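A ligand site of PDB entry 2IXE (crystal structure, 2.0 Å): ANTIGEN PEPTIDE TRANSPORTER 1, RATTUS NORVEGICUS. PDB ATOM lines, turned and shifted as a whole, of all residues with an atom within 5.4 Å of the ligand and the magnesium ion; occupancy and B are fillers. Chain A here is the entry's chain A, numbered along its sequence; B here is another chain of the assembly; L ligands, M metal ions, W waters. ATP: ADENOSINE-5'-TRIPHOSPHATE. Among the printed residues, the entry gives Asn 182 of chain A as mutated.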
ATOM      1  N   TYR A  26      27.900 -12.660  28.641  1.00  0.00           N
ATOM      2  CA  TYR A  26      29.021 -13.383  29.231  1.00  0.00           C
ATOM      3  C   TYR A  26      30.087 -12.404  29.712  1.00  0.00           C
ATOM      4  O   TYR A  26      30.386 -11.434  29.025  1.00  0.00           O
ATOM      5  CB  TYR A  26      29.605 -14.410  28.259  1.00  0.00           C
ATOM      6  CG  TYR A  26      28.721 -15.613  28.155  1.00  0.00           C
ATOM      7  CD1 TYR A  26      27.720 -15.686  27.188  1.00  0.00           C
ATOM      8  CD2 TYR A  26      28.833 -16.665  29.056  1.00  0.00           C
ATOM      9  CE1 TYR A  26      26.890 -16.786  27.107  1.00  0.00           C
ATOM     10  CE2 TYR A  26      28.008 -17.762  28.988  1.00  0.00           C
ATOM     11  CZ  TYR A  26      27.043 -17.823  28.003  1.00  0.00           C
ATOM     12  OH  TYR A  26      26.197 -18.925  27.929  1.00  0.00           O
ATOM     13  N   HIS A  29      32.582 -11.092  27.365  1.00  0.00           N
ATOM     14  CA  HIS A  29      31.989 -10.494  26.168  1.00  0.00           C
ATOM     15  C   HIS A  29      30.798  -9.596  26.565  1.00  0.00           C
ATOM     16  O   HIS A  29      29.650  -9.883  26.201  1.00  0.00           O
ATOM     17  CB  HIS A  29      31.533 -11.574  25.189  1.00  0.00           C
ATOM     18  CG  HIS A  29      32.656 -12.299  24.523  1.00  0.00           C
ATOM     19  ND1 HIS A  29      33.375 -11.756  23.474  1.00  0.00           N
ATOM     20  CD2 HIS A  29      33.186 -13.526  24.747  1.00  0.00           C
ATOM     21  CE1 HIS A  29      34.308 -12.616  23.088  1.00  0.00           C
ATOM     22  NE2 HIS A  29      34.206 -13.694  23.844  1.00  0.00           N
ATOM     23  N   VAL A  34      22.978 -11.557  25.433  1.00  0.00           N
ATOM     24  CA  VAL A  34      22.522 -12.909  25.188  1.00  0.00           C
ATOM     25  C   VAL A  34      21.085 -13.036  25.657  1.00  0.00           C
ATOM     26  O   VAL A  34      20.205 -13.460  24.906  1.00  0.00           O
ATOM     27  CB  VAL A  34      23.410 -13.951  25.888  1.00  0.00           C
ATOM     28  CG1 VAL A  34      22.849 -15.344  25.709  1.00  0.00           C
ATOM     29  CG2 VAL A  34      24.843 -13.876  25.347  1.00  0.00           C
ATOM     30  N   GLY A  52      13.221 -22.835  20.744  1.00  0.00           N
ATOM     31  CA  GLY A  52      13.564 -21.647  19.976  1.00  0.00           C
ATOM     32  C   GLY A  52      14.792 -21.851  19.127  1.00  0.00           C
ATOM     33  O   GLY A  52      15.497 -22.854  19.287  1.00  0.00           O
ATOM     34  N   PRO A  53      15.075 -20.886  18.245  1.00  0.00           N
ATOM     35  CA  PRO A  53      16.148 -21.035  17.278  1.00  0.00           C
ATOM     36  C   PRO A  53      17.540 -21.121  17.902  1.00  0.00           C
ATOM     37  O   PRO A  53      17.749 -20.778  19.074  1.00  0.00           O
ATOM     38  CB  PRO A  53      16.012 -19.792  16.384  1.00  0.00           C
ATOM     39  CG  PRO A  53      15.226 -18.832  17.155  1.00  0.00           C
ATOM     40  CD  PRO A  53      14.379 -19.593  18.107  1.00  0.00           C
ATOM     41  N   ASN A  54      18.481 -21.604  17.088  1.00  0.00           N
ATOM     42  CA  ASN A  54      19.862 -21.760  17.485  1.00  0.00           C
ATOM     43  C   ASN A  54      20.429 -20.400  17.865  1.00  0.00           C
ATOM     44  O   ASN A  54      20.215 -19.420  17.155  1.00  0.00           O
ATOM     45  CB  ASN A  54      20.687 -22.369  16.342  1.00  0.00           C
ATOM     46  CG  ASN A  54      20.250 -23.794  16.000  1.00  0.00           C
ATOM     47  OD1 ASN A  54      20.156 -24.154  14.827  1.00  0.00           O
ATOM     48  ND2 ASN A  54      19.977 -24.609  17.019  1.00  0.00           N
ATOM     49  N   GLY A  55      21.118 -20.337  19.002  1.00  0.00           N
ATOM     50  CA  GLY A  55      21.685 -19.089  19.504  1.00  0.00           C
ATOM     51  C   GLY A  55      20.732 -18.188  20.262  1.00  0.00           C
ATOM     52  O   GLY A  55      21.126 -17.098  20.684  1.00  0.00           O
ATOM     53  N   SER A  56      19.485 -18.608  20.446  1.00  0.00           N
ATOM     54  CA  SER A  56      18.488 -17.761  21.116  1.00  0.00           C
ATOM     55  C   SER A  56      18.764 -17.556  22.610  1.00  0.00           C
ATOM     56  O   SER A  56      18.286 -16.576  23.203  1.00  0.00           O
ATOM     57  CB  SER A  56      17.048 -18.285  20.911  1.00  0.00           C
ATOM     58  OG  SER A  56      16.864 -19.596  21.423  1.00  0.00           O
ATOM     59  N   GLY A  57      19.543 -18.457  23.222  1.00  0.00           N
ATOM     60  CA  GLY A  57      19.931 -18.307  24.624  1.00  0.00           C
ATOM     61  C   GLY A  57      19.477 -19.415  25.570  1.00  0.00           C
ATOM     62  O   GLY A  57      19.632 -19.290  26.780  1.00  0.00           O
ATOM     63  N   LYS A  58      18.976 -20.518  25.005  1.00  0.00           N
ATOM     64  CA  LYS A  58      18.401 -21.600  25.803  1.00  0.00           C
ATOM     65  C   LYS A  58      19.411 -22.260  26.747  1.00  0.00           C
ATOM     66  O   LYS A  58      19.152 -22.414  27.947  1.00  0.00           O
ATOM     67  CB  LYS A  58      17.789 -22.657  24.879  1.00  0.00           C
ATOM     68  CG  LYS A  58      16.704 -22.129  23.959  1.00  0.00           C
ATOM     69  CD  LYS A  58      16.080 -23.235  23.099  1.00  0.00           C
ATOM     70  CE  LYS A  58      17.095 -23.920  22.168  1.00  0.00           C
ATOM     71  NZ  LYS A  58      17.677 -22.989  21.164  1.00  0.00           N
ATOM     72  N   SER A  59      20.567 -22.626  26.210  1.00  0.00           N
ATOM     73  CA  SER A  59      21.629 -23.211  27.028  1.00  0.00           C
ATOM     74  C   SER A  59      22.201 -22.199  28.026  1.00  0.00           C
ATOM     75  O   SER A  59      22.663 -22.578  29.101  1.00  0.00           O
ATOM     76  CB  SER A  59      22.747 -23.798  26.157  1.00  0.00           C
ATOM     77  OG  SER A  59      22.255 -24.880  25.380  1.00  0.00           O
ATOM     78  N   THR A  60      22.163 -20.914  27.684  1.00  0.00           N
ATOM     79  CA  THR A  60      22.599 -19.861  28.607  1.00  0.00           C
ATOM     80  C   THR A  60      21.623 -19.799  29.802  1.00  0.00           C
ATOM     81  O   THR A  60      22.056 -19.638  30.950  1.00  0.00           O
ATOM     82  CB  THR A  60      22.740 -18.492  27.886  1.00  0.00           C
ATOM     83  OG1 THR A  60      23.779 -18.574  26.899  1.00  0.00           O
ATOM     84  CG2 THR A  60      23.105 -17.377  28.851  1.00  0.00           C
ATOM     85  N   VAL A  61      20.341 -19.951  29.532  1.00  0.00           N
ATOM     86  CA  VAL A  61      19.332 -20.012  30.599  1.00  0.00           C
ATOM     87  C   VAL A  61      19.622 -21.203  31.530  1.00  0.00           C
ATOM     88  O   VAL A  61      19.585 -21.070  32.749  1.00  0.00           O
ATOM     89  CB  VAL A  61      17.895 -20.073  30.023  1.00  0.00           C
ATOM     90  CG1 VAL A  61      16.876 -20.388  31.121  1.00  0.00           C
ATOM     91  CG2 VAL A  61      17.538 -18.762  29.329  1.00  0.00           C
ATOM     92  N   TYR A  69      26.681 -18.774  36.210  1.00  0.00           N
ATOM     93  CA  TYR A  69      26.870 -17.336  36.076  1.00  0.00           C
ATOM     94  C   TYR A  69      25.716 -16.652  36.780  1.00  0.00           C
ATOM     95  O   TYR A  69      24.695 -17.284  37.088  1.00  0.00           O
ATOM     96  CB  TYR A  69      26.868 -16.924  34.605  1.00  0.00           C
ATOM     97  CG  TYR A  69      27.794 -17.721  33.730  1.00  0.00           C
ATOM     98  CD1 TYR A  69      29.083 -17.270  33.444  1.00  0.00           C
ATOM     99  CD2 TYR A  69      27.391 -18.934  33.179  1.00  0.00           C
ATOM    100  CE1 TYR A  69      29.935 -18.005  32.636  1.00  0.00           C
ATOM    101  CE2 TYR A  69      28.231 -19.662  32.374  1.00  0.00           C
ATOM    102  CZ  TYR A  69      29.501 -19.195  32.106  1.00  0.00           C
ATOM    103  OH  TYR A  69      30.333 -19.940  31.308  1.00  0.00           O
ATOM    104  N   ASP A 181      19.064 -30.604  28.501  1.00  0.00           N
ATOM    105  CA  ASP A 181      19.449 -29.761  27.362  1.00  0.00           C
ATOM    106  C   ASP A 181      19.889 -30.602  26.155  1.00  0.00           C
ATOM    107  O   ASP A 181      21.042 -31.018  26.068  1.00  0.00           O
ATOM    108  CB  ASP A 181      20.554 -28.798  27.770  1.00  0.00           C
ATOM    109  CG  ASP A 181      20.813 -27.716  26.726  1.00  0.00           C
ATOM    110  OD1 ASP A 181      20.212 -27.788  25.635  1.00  0.00           O
ATOM    111  OD2 ASP A 181      21.616 -26.798  27.013  1.00  0.00           O
ATOM    112  N   ASN A 182      18.964 -30.836  25.223  1.00  0.00           N
ATOM    113  CA  ASN A 182      19.163 -31.788  24.131  1.00  0.00           C
ATOM    114  C   ASN A 182      19.652 -33.134  24.666  1.00  0.00           C
ATOM    115  O   ASN A 182      20.462 -33.797  24.034  1.00  0.00           O
ATOM    116  CB  ASN A 182      20.173 -31.264  23.099  1.00  0.00           C
ATOM    117  CG  ASN A 182      19.736 -29.984  22.413  1.00  0.00           C
ATOM    118  OD1 ASN A 182      18.550 -29.693  22.311  1.00  0.00           O
ATOM    119  ND2 ASN A 182      20.707 -29.211  21.915  1.00  0.00           N
ATOM    120  N   ILE A 213      14.766 -28.587  27.318  1.00  0.00           N
ATOM    121  CA  ILE A 213      15.251 -27.862  26.147  1.00  0.00           C
ATOM    122  C   ILE A 213      15.459 -28.852  25.006  1.00  0.00           C
ATOM    123  O   ILE A 213      16.172 -29.843  25.176  1.00  0.00           O
ATOM    124  CB  ILE A 213      16.586 -27.148  26.438  1.00  0.00           C
ATOM    125  CG1 ILE A 213      16.411 -26.146  27.586  1.00  0.00           C
ATOM    126  CG2 ILE A 213      17.118 -26.461  25.173  1.00  0.00           C
ATOM    127  CD1 ILE A 213      17.706 -25.682  28.183  1.00  0.00           C
ATOM    128  N   GLN A 215      15.152 -29.330  20.345  1.00  0.00           N
ATOM    129  CA  GLN A 215      14.750 -28.919  18.997  1.00  0.00           C
ATOM    130  C   GLN A 215      13.711 -29.868  18.420  1.00  0.00           C
ATOM    131  O   GLN A 215      13.137 -29.582  17.366  1.00  0.00           O
ATOM    132  CB  GLN A 215      15.978 -28.843  18.083  1.00  0.00           C
ATOM    133  CG  GLN A 215      16.971 -27.744  18.468  1.00  0.00           C
ATOM    134  CD  GLN A 215      16.391 -26.342  18.351  1.00  0.00           C
ATOM    135  OE1 GLN A 215      15.292 -26.144  17.826  1.00  0.00           O
ATOM    136  NE2 GLN A 215      17.149 -25.361  18.818  1.00  0.00           N
ATOM    137  N   LEU A 229      11.742 -19.019  23.162  1.00  0.00           N
ATOM    138  CA  LEU A 229      12.802 -18.032  23.331  1.00  0.00           C
ATOM    139  C   LEU A 229      13.291 -17.545  21.972  1.00  0.00           C
ATOM    140  O   LEU A 229      13.598 -18.350  21.088  1.00  0.00           O
ATOM    141  CB  LEU A 229      13.945 -18.641  24.125  1.00  0.00           C
ATOM    142  CG  LEU A 229      15.007 -17.710  24.737  1.00  0.00           C
ATOM    143  CD1 LEU A 229      14.479 -17.014  25.984  1.00  0.00           C
ATOM    144  CD2 LEU A 229      16.247 -18.499  25.080  1.00  0.00           C
ATOM    145  N   PHE B 142      29.801 -11.585  14.460  1.00  0.00           N
ATOM    146  CA  PHE B 142      31.051 -11.227  15.118  1.00  0.00           C
ATOM    147  C   PHE B 142      31.703 -10.048  14.381  1.00  0.00           C
ATOM    148  O   PHE B 142      31.596  -9.963  13.160  1.00  0.00           O
ATOM    149  CB  PHE B 142      32.034 -12.407  15.162  1.00  0.00           C
ATOM    150  CG  PHE B 142      31.528 -13.592  15.930  1.00  0.00           C
ATOM    151  CD1 PHE B 142      31.200 -13.485  17.276  1.00  0.00           C
ATOM    152  CD2 PHE B 142      31.400 -14.836  15.320  1.00  0.00           C
ATOM    153  CE1 PHE B 142      30.739 -14.582  17.995  1.00  0.00           C
ATOM    154  CE2 PHE B 142      30.946 -15.943  16.023  1.00  0.00           C
ATOM    155  CZ  PHE B 142      30.614 -15.813  17.365  1.00  0.00           C
ATOM    156  N   GLN B 156      31.990 -18.302  22.744  1.00  0.00           N
ATOM    157  CA  GLN B 156      31.896 -19.714  22.382  1.00  0.00           C
ATOM    158  C   GLN B 156      30.558 -19.982  21.704  1.00  0.00           C
ATOM    159  O   GLN B 156      29.680 -19.118  21.694  1.00  0.00           O
ATOM    160  CB  GLN B 156      32.091 -20.598  23.621  1.00  0.00           C
ATOM    161  CG  GLN B 156      33.552 -20.713  24.116  1.00  0.00           C
ATOM    162  CD  GLN B 156      34.020 -19.541  24.965  1.00  0.00           C
ATOM    163  OE1 GLN B 156      33.877 -18.382  24.579  1.00  0.00           O
ATOM    164  NE2 GLN B 156      34.585 -19.847  26.129  1.00  0.00           N
ATOM    165  N   LEU B 157      30.399 -21.176  21.124  1.00  0.00           N
ATOM    166  CA  LEU B 157      29.250 -21.475  20.272  1.00  0.00           C
ATOM    167  C   LEU B 157      28.153 -22.248  20.966  1.00  0.00           C
ATOM    168  O   LEU B 157      28.389 -22.912  21.967  1.00  0.00           O
ATOM    169  CB  LEU B 157      29.689 -22.265  19.045  1.00  0.00           C
ATOM    170  CG  LEU B 157      30.742 -21.611  18.166  1.00  0.00           C
ATOM    171  CD1 LEU B 157      30.851 -22.341  16.839  1.00  0.00           C
ATOM    172  CD2 LEU B 157      30.414 -20.135  17.963  1.00  0.00           C
ATOM    173  N   SER B 158      26.945 -22.143  20.414  1.00  0.00           N
ATOM    174  CA  SER B 158      25.832 -22.962  20.876  1.00  0.00           C
ATOM    175  C   SER B 158      25.931 -24.329  20.218  1.00  0.00           C
ATOM    176  O   SER B 158      26.685 -24.519  19.260  1.00  0.00           O
ATOM    177  CB  SER B 158      24.499 -22.283  20.535  1.00  0.00           C
ATOM    178  OG  SER B 158      24.246 -22.326  19.139  1.00  0.00           O
ATOM    179  N   GLY B 159      25.166 -25.292  20.740  1.00  0.00           N
ATOM    180  CA  GLY B 159      25.165 -26.648  20.195  1.00  0.00           C
ATOM    181  C   GLY B 159      24.853 -26.714  18.711  1.00  0.00           C
ATOM    182  O   GLY B 159      25.532 -27.396  17.955  1.00  0.00           O
ATOM    183  N   GLY B 160      23.813 -25.998  18.302  1.00  0.00           N
ATOM    184  CA  GLY B 160      23.405 -25.948  16.903  1.00  0.00           C
ATOM    185  C   GLY B 160      24.391 -25.218  16.021  1.00  0.00           C
ATOM    186  O   GLY B 160      24.627 -25.608  14.878  1.00  0.00           O
ATOM    187  N   GLN B 161      24.972 -24.146  16.540  1.00  0.00           N
ATOM    188  CA  GLN B 161      26.006 -23.397  15.807  1.00  0.00           C
ATOM    189  C   GLN B 161      27.238 -24.266  15.550  1.00  0.00           C
ATOM    190  O   GLN B 161      27.783 -24.241  14.460  1.00  0.00           O
ATOM    191  CB  GLN B 161      26.388 -22.125  16.554  1.00  0.00           C
ATOM    192  CG  GLN B 161      25.310 -21.037  16.500  1.00  0.00           C
ATOM    193  CD  GLN B 161      25.542 -19.907  17.497  1.00  0.00           C
ATOM    194  OE1 GLN B 161      26.434 -19.979  18.342  1.00  0.00           O
ATOM    195  NE2 GLN B 161      24.709 -18.877  17.426  1.00  0.00           N
ATOM    196  N   ALA B 186      20.976 -31.017  16.940  1.00  0.00           N
ATOM    197  CA  ALA B 186      20.883 -29.748  17.675  1.00  0.00           C
ATOM    198  C   ALA B 186      20.385 -28.575  16.814  1.00  0.00           C
ATOM    199  O   ALA B 186      20.143 -27.496  17.337  1.00  0.00           O
ATOM    200  CB  ALA B 186      22.237 -29.408  18.290  1.00  0.00           C
HETATM  201  PG  ATP L   1      21.220 -23.991  20.340  1.00  0.00           P
HETATM  202  O1G ATP L   1      19.757 -24.209  20.055  1.00  0.00           O
HETATM  203  O2G ATP L   1      22.066 -23.882  19.104  1.00  0.00           O
HETATM  204  O3G ATP L   1      21.766 -24.882  21.437  1.00  0.00           O
HETATM  205  PB  ATP L   1      21.009 -21.944  22.392  1.00  0.00           P
HETATM  206  O1B ATP L   1      19.618 -21.348  22.345  1.00  0.00           O
HETATM  207  O2B ATP L   1      21.281 -22.939  23.482  1.00  0.00           O
HETATM  208  O3B ATP L   1      21.361 -22.465  20.903  1.00  0.00           O
HETATM  209  PA  ATP L   1      23.206 -20.534  23.659  1.00  0.00           P
HETATM  210  O1A ATP L   1      22.523 -20.138  24.951  1.00  0.00           O
HETATM  211  O2A ATP L   1      24.172 -21.706  23.677  1.00  0.00           O
HETATM  212  O3A ATP L   1      22.093 -20.718  22.483  1.00  0.00           O
HETATM  213  O5' ATP L   1      24.051 -19.300  23.115  1.00  0.00           O
HETATM  214  C5' ATP L   1      23.551 -17.965  23.141  1.00  0.00           C
HETATM  215  C4' ATP L   1      24.631 -17.051  22.565  1.00  0.00           C
HETATM  216  O4' ATP L   1      25.701 -16.967  23.519  1.00  0.00           O
HETATM  217  C3' ATP L   1      25.221 -17.603  21.280  1.00  0.00           C
HETATM  218  O3' ATP L   1      25.324 -16.584  20.282  1.00  0.00           O
HETATM  219  C2' ATP L   1      26.586 -18.138  21.657  1.00  0.00           C
HETATM  220  O2' ATP L   1      27.508 -17.907  20.594  1.00  0.00           O
HETATM  221  C1' ATP L   1      26.938 -17.351  22.915  1.00  0.00           C
HETATM  222  N9  ATP L   1      27.712 -18.110  23.929  1.00  0.00           N
HETATM  223  C8  ATP L   1      27.395 -19.323  24.421  1.00  0.00           C
HETATM  224  N7  ATP L   1      28.305 -19.709  25.348  1.00  0.00           N
HETATM  225  C5  ATP L   1      29.219 -18.726  25.465  1.00  0.00           C
HETATM  226  C6  ATP L   1      30.450 -18.491  26.256  1.00  0.00           C
HETATM  227  N6  ATP L   1      30.891 -19.417  27.137  1.00  0.00           N
HETATM  228  N1  ATP L   1      31.106 -17.321  26.073  1.00  0.00           N
HETATM  229  C2  ATP L   1      30.677 -16.388  25.193  1.00  0.00           C
HETATM  230  N3  ATP L   1      29.580 -16.549  24.442  1.00  0.00           N
HETATM  231  C4  ATP L   1      28.814 -17.664  24.527  1.00  0.00           C
HETATM  232 MG    MG M   1      21.922 -25.006  23.327  1.00  0.00          MG
HETATM  233  O   HOH W   1      20.144 -25.875  23.582  1.00  0.00           O
HETATM  234  O   HOH W   2      26.122 -22.428  25.647  1.00  0.00           O
HETATM  235  O   HOH W   3      23.150 -26.871  23.462  1.00  0.00           O
HETATM  236  O   HOH W   4      19.918 -26.924  19.919  1.00  0.00           O
HETATM  237  O   HOH W   5      28.506 -14.048  23.894  1.00  0.00           O
HETATM  238  O   HOH W   6      33.136 -16.188  27.835  1.00  0.00           O
HETATM  239  O   HOH W   7      23.855 -24.329  23.201  1.00  0.00           O
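The side-chain hydroxyl (OG) of Ser 59 sits close to the side-chain carboxylate (OD2) of Asp 181 (2.6 Å). The side-chain amide nitrogen (NE2) of Gln 215 sits close to the side-chain amino group (NZ) of Lys 58, 3.4 Å away. OG of Ser 56 lies within hydrogen-bond range of NZ of Lys 58 (3.5 Å). O of Pro 53 sits at hydrogen-bond distance from NZ of Lys 58, at 3.0 Å. The side-chain amino group (NZ) of Lys 58 sits at hydrogen-bond distance from the backbone carbonyl oxygen (O) of Gly 52, at 2.9 Å. OG1 of Thr 60 sits at hydrogen-bond distance from OH of Tyr 26 (2.7 Å). The side-chain amide nitrogen (ND2) of Asn 54 is in hydrogen-bond range of the backbone carbonyl oxygen (O) of Ala 186 of chain B. OG of Ser 56 is in hydrogen-bond range of O of Pro 53, at 2.8 Å.
Water W7 bridges an oxygen (O2A) of the ligand and the backbone NH (N) of Gly 159 of chain B. Water W4 lies within hydrogen-bond range of the backbone carbonyl oxygen (O) of Ala 186 of chain B, an oxygen (O1G) of the ligand, the side-chain amide nitrogen (ND2) of Asn 182 and the side-chain amide nitrogen (NE2) of Gln 215.
The magnesium ion is bound by O3G of the ligand (1.9 Å). The magnesium ion is bound by water W1 (2.0 Å). Water W7 binds the magnesium ion (2.1 Å). The side-chain hydroxyl (OG) of Ser 59 binds the magnesium ion (2.1 Å). O2B of the ligand is bound to the magnesium ion (2.2 Å). Water W3 is bound to the magnesium ion, at 2.2 Å.
The backbone NH of Ser 59 lies within hydrogen-bond range of an oxygen (O1A) of the ligand (3.4 Å). N of Lys 58 is in hydrogen-bond range of O1B of the ligand, at 2.9 Å. O1G of the ligand lies within salt-bridge range of NZ of Lys 58. The side-chain hydroxyl (OG) of Ser 158 of chain B is in hydrogen-bond range of an oxygen (O2G) of the ligand (2.7 Å). A nitrogen (N3) of the ligand sits close to the backbone NH (N) of Gln 156 of chain B (3.4 Å). O of Gln 156 of chain B sits at hydrogen-bond distance from O2' of the ligand (2.7 Å). The side-chain amide oxygen (OE1) of Gln 156 of chain B lies close to a nitrogen (N1) of the ligand (3.3 Å). The backbone NH of Thr 60 sits at hydrogen-bond distance from an oxygen (O1A) of the ligand (2.9 Å). The side-chain hydroxyl (OG1) of Thr 60 sits at hydrogen-bond distance from an oxygen (O1A) of the ligand, 2.8 Å away. The backbone NH (N) of Gly 160 of chain B lies within hydrogen-bond range of an oxygen (O2G) of the ligand (2.9 Å). An oxygen (O3B) of the ligand sits at hydrogen-bond distance from the backbone NH (N) of Gly 55. The backbone NH (N) of Gly 57 is in hydrogen-bond range of an oxygen (O1B) of the ligand, at 3.0 Å. ND2 of Asn 54 lies within hydrogen-bond range of O2G of the ligand (3.0 Å). NE2 of Gln 215 lies within hydrogen-bond range of O1G of the ligand. The side-chain amide oxygen (OE1) of Gln 161 of chain B lies within hydrogen-bond range of an oxygen (O2') of the ligand, 3.2 Å away. A nitrogen (N7) of the ligand is in hydrogen-bond range of the side-chain hydroxyl (OH) of Tyr 26 (3.4 Å). The backbone NH of Ser 56 sits at hydrogen-bond distance from an oxygen (O1B) of the ligand, at 3.3 Å. An oxygen (O1B) of the ligand is in hydrogen-bond range of the side-chain hydroxyl (OG) of Ser 56 (3.4 Å). N of Gly 159 of chain B sits close to O3G of the ligand (3.5 Å).
Asp 181 touches the magnesium ion. Within 4 Å of the magnesium ion: Ser 59 and Asp 181.
Merely in contact with the ligand: His 29, Val 34, Pro 53 and Leu 157 of chain B. Within 4 Å of the ligand: Tyr 26, His 29, Val 34, Pro 53, Asn 54, Gly 55, Ser 56, Gly 57, Lys 58, Ser 59, Thr 60, Gln 215, Gln 156 of chain B, Leu 157 of chain B, Ser 158 of chain B, Gly 159 of chain B, Gly 160 of chain B and Gln 161 of chain B. The nearest printed residue that does not touch the ligand is Tyr 69 (4.2 Å).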
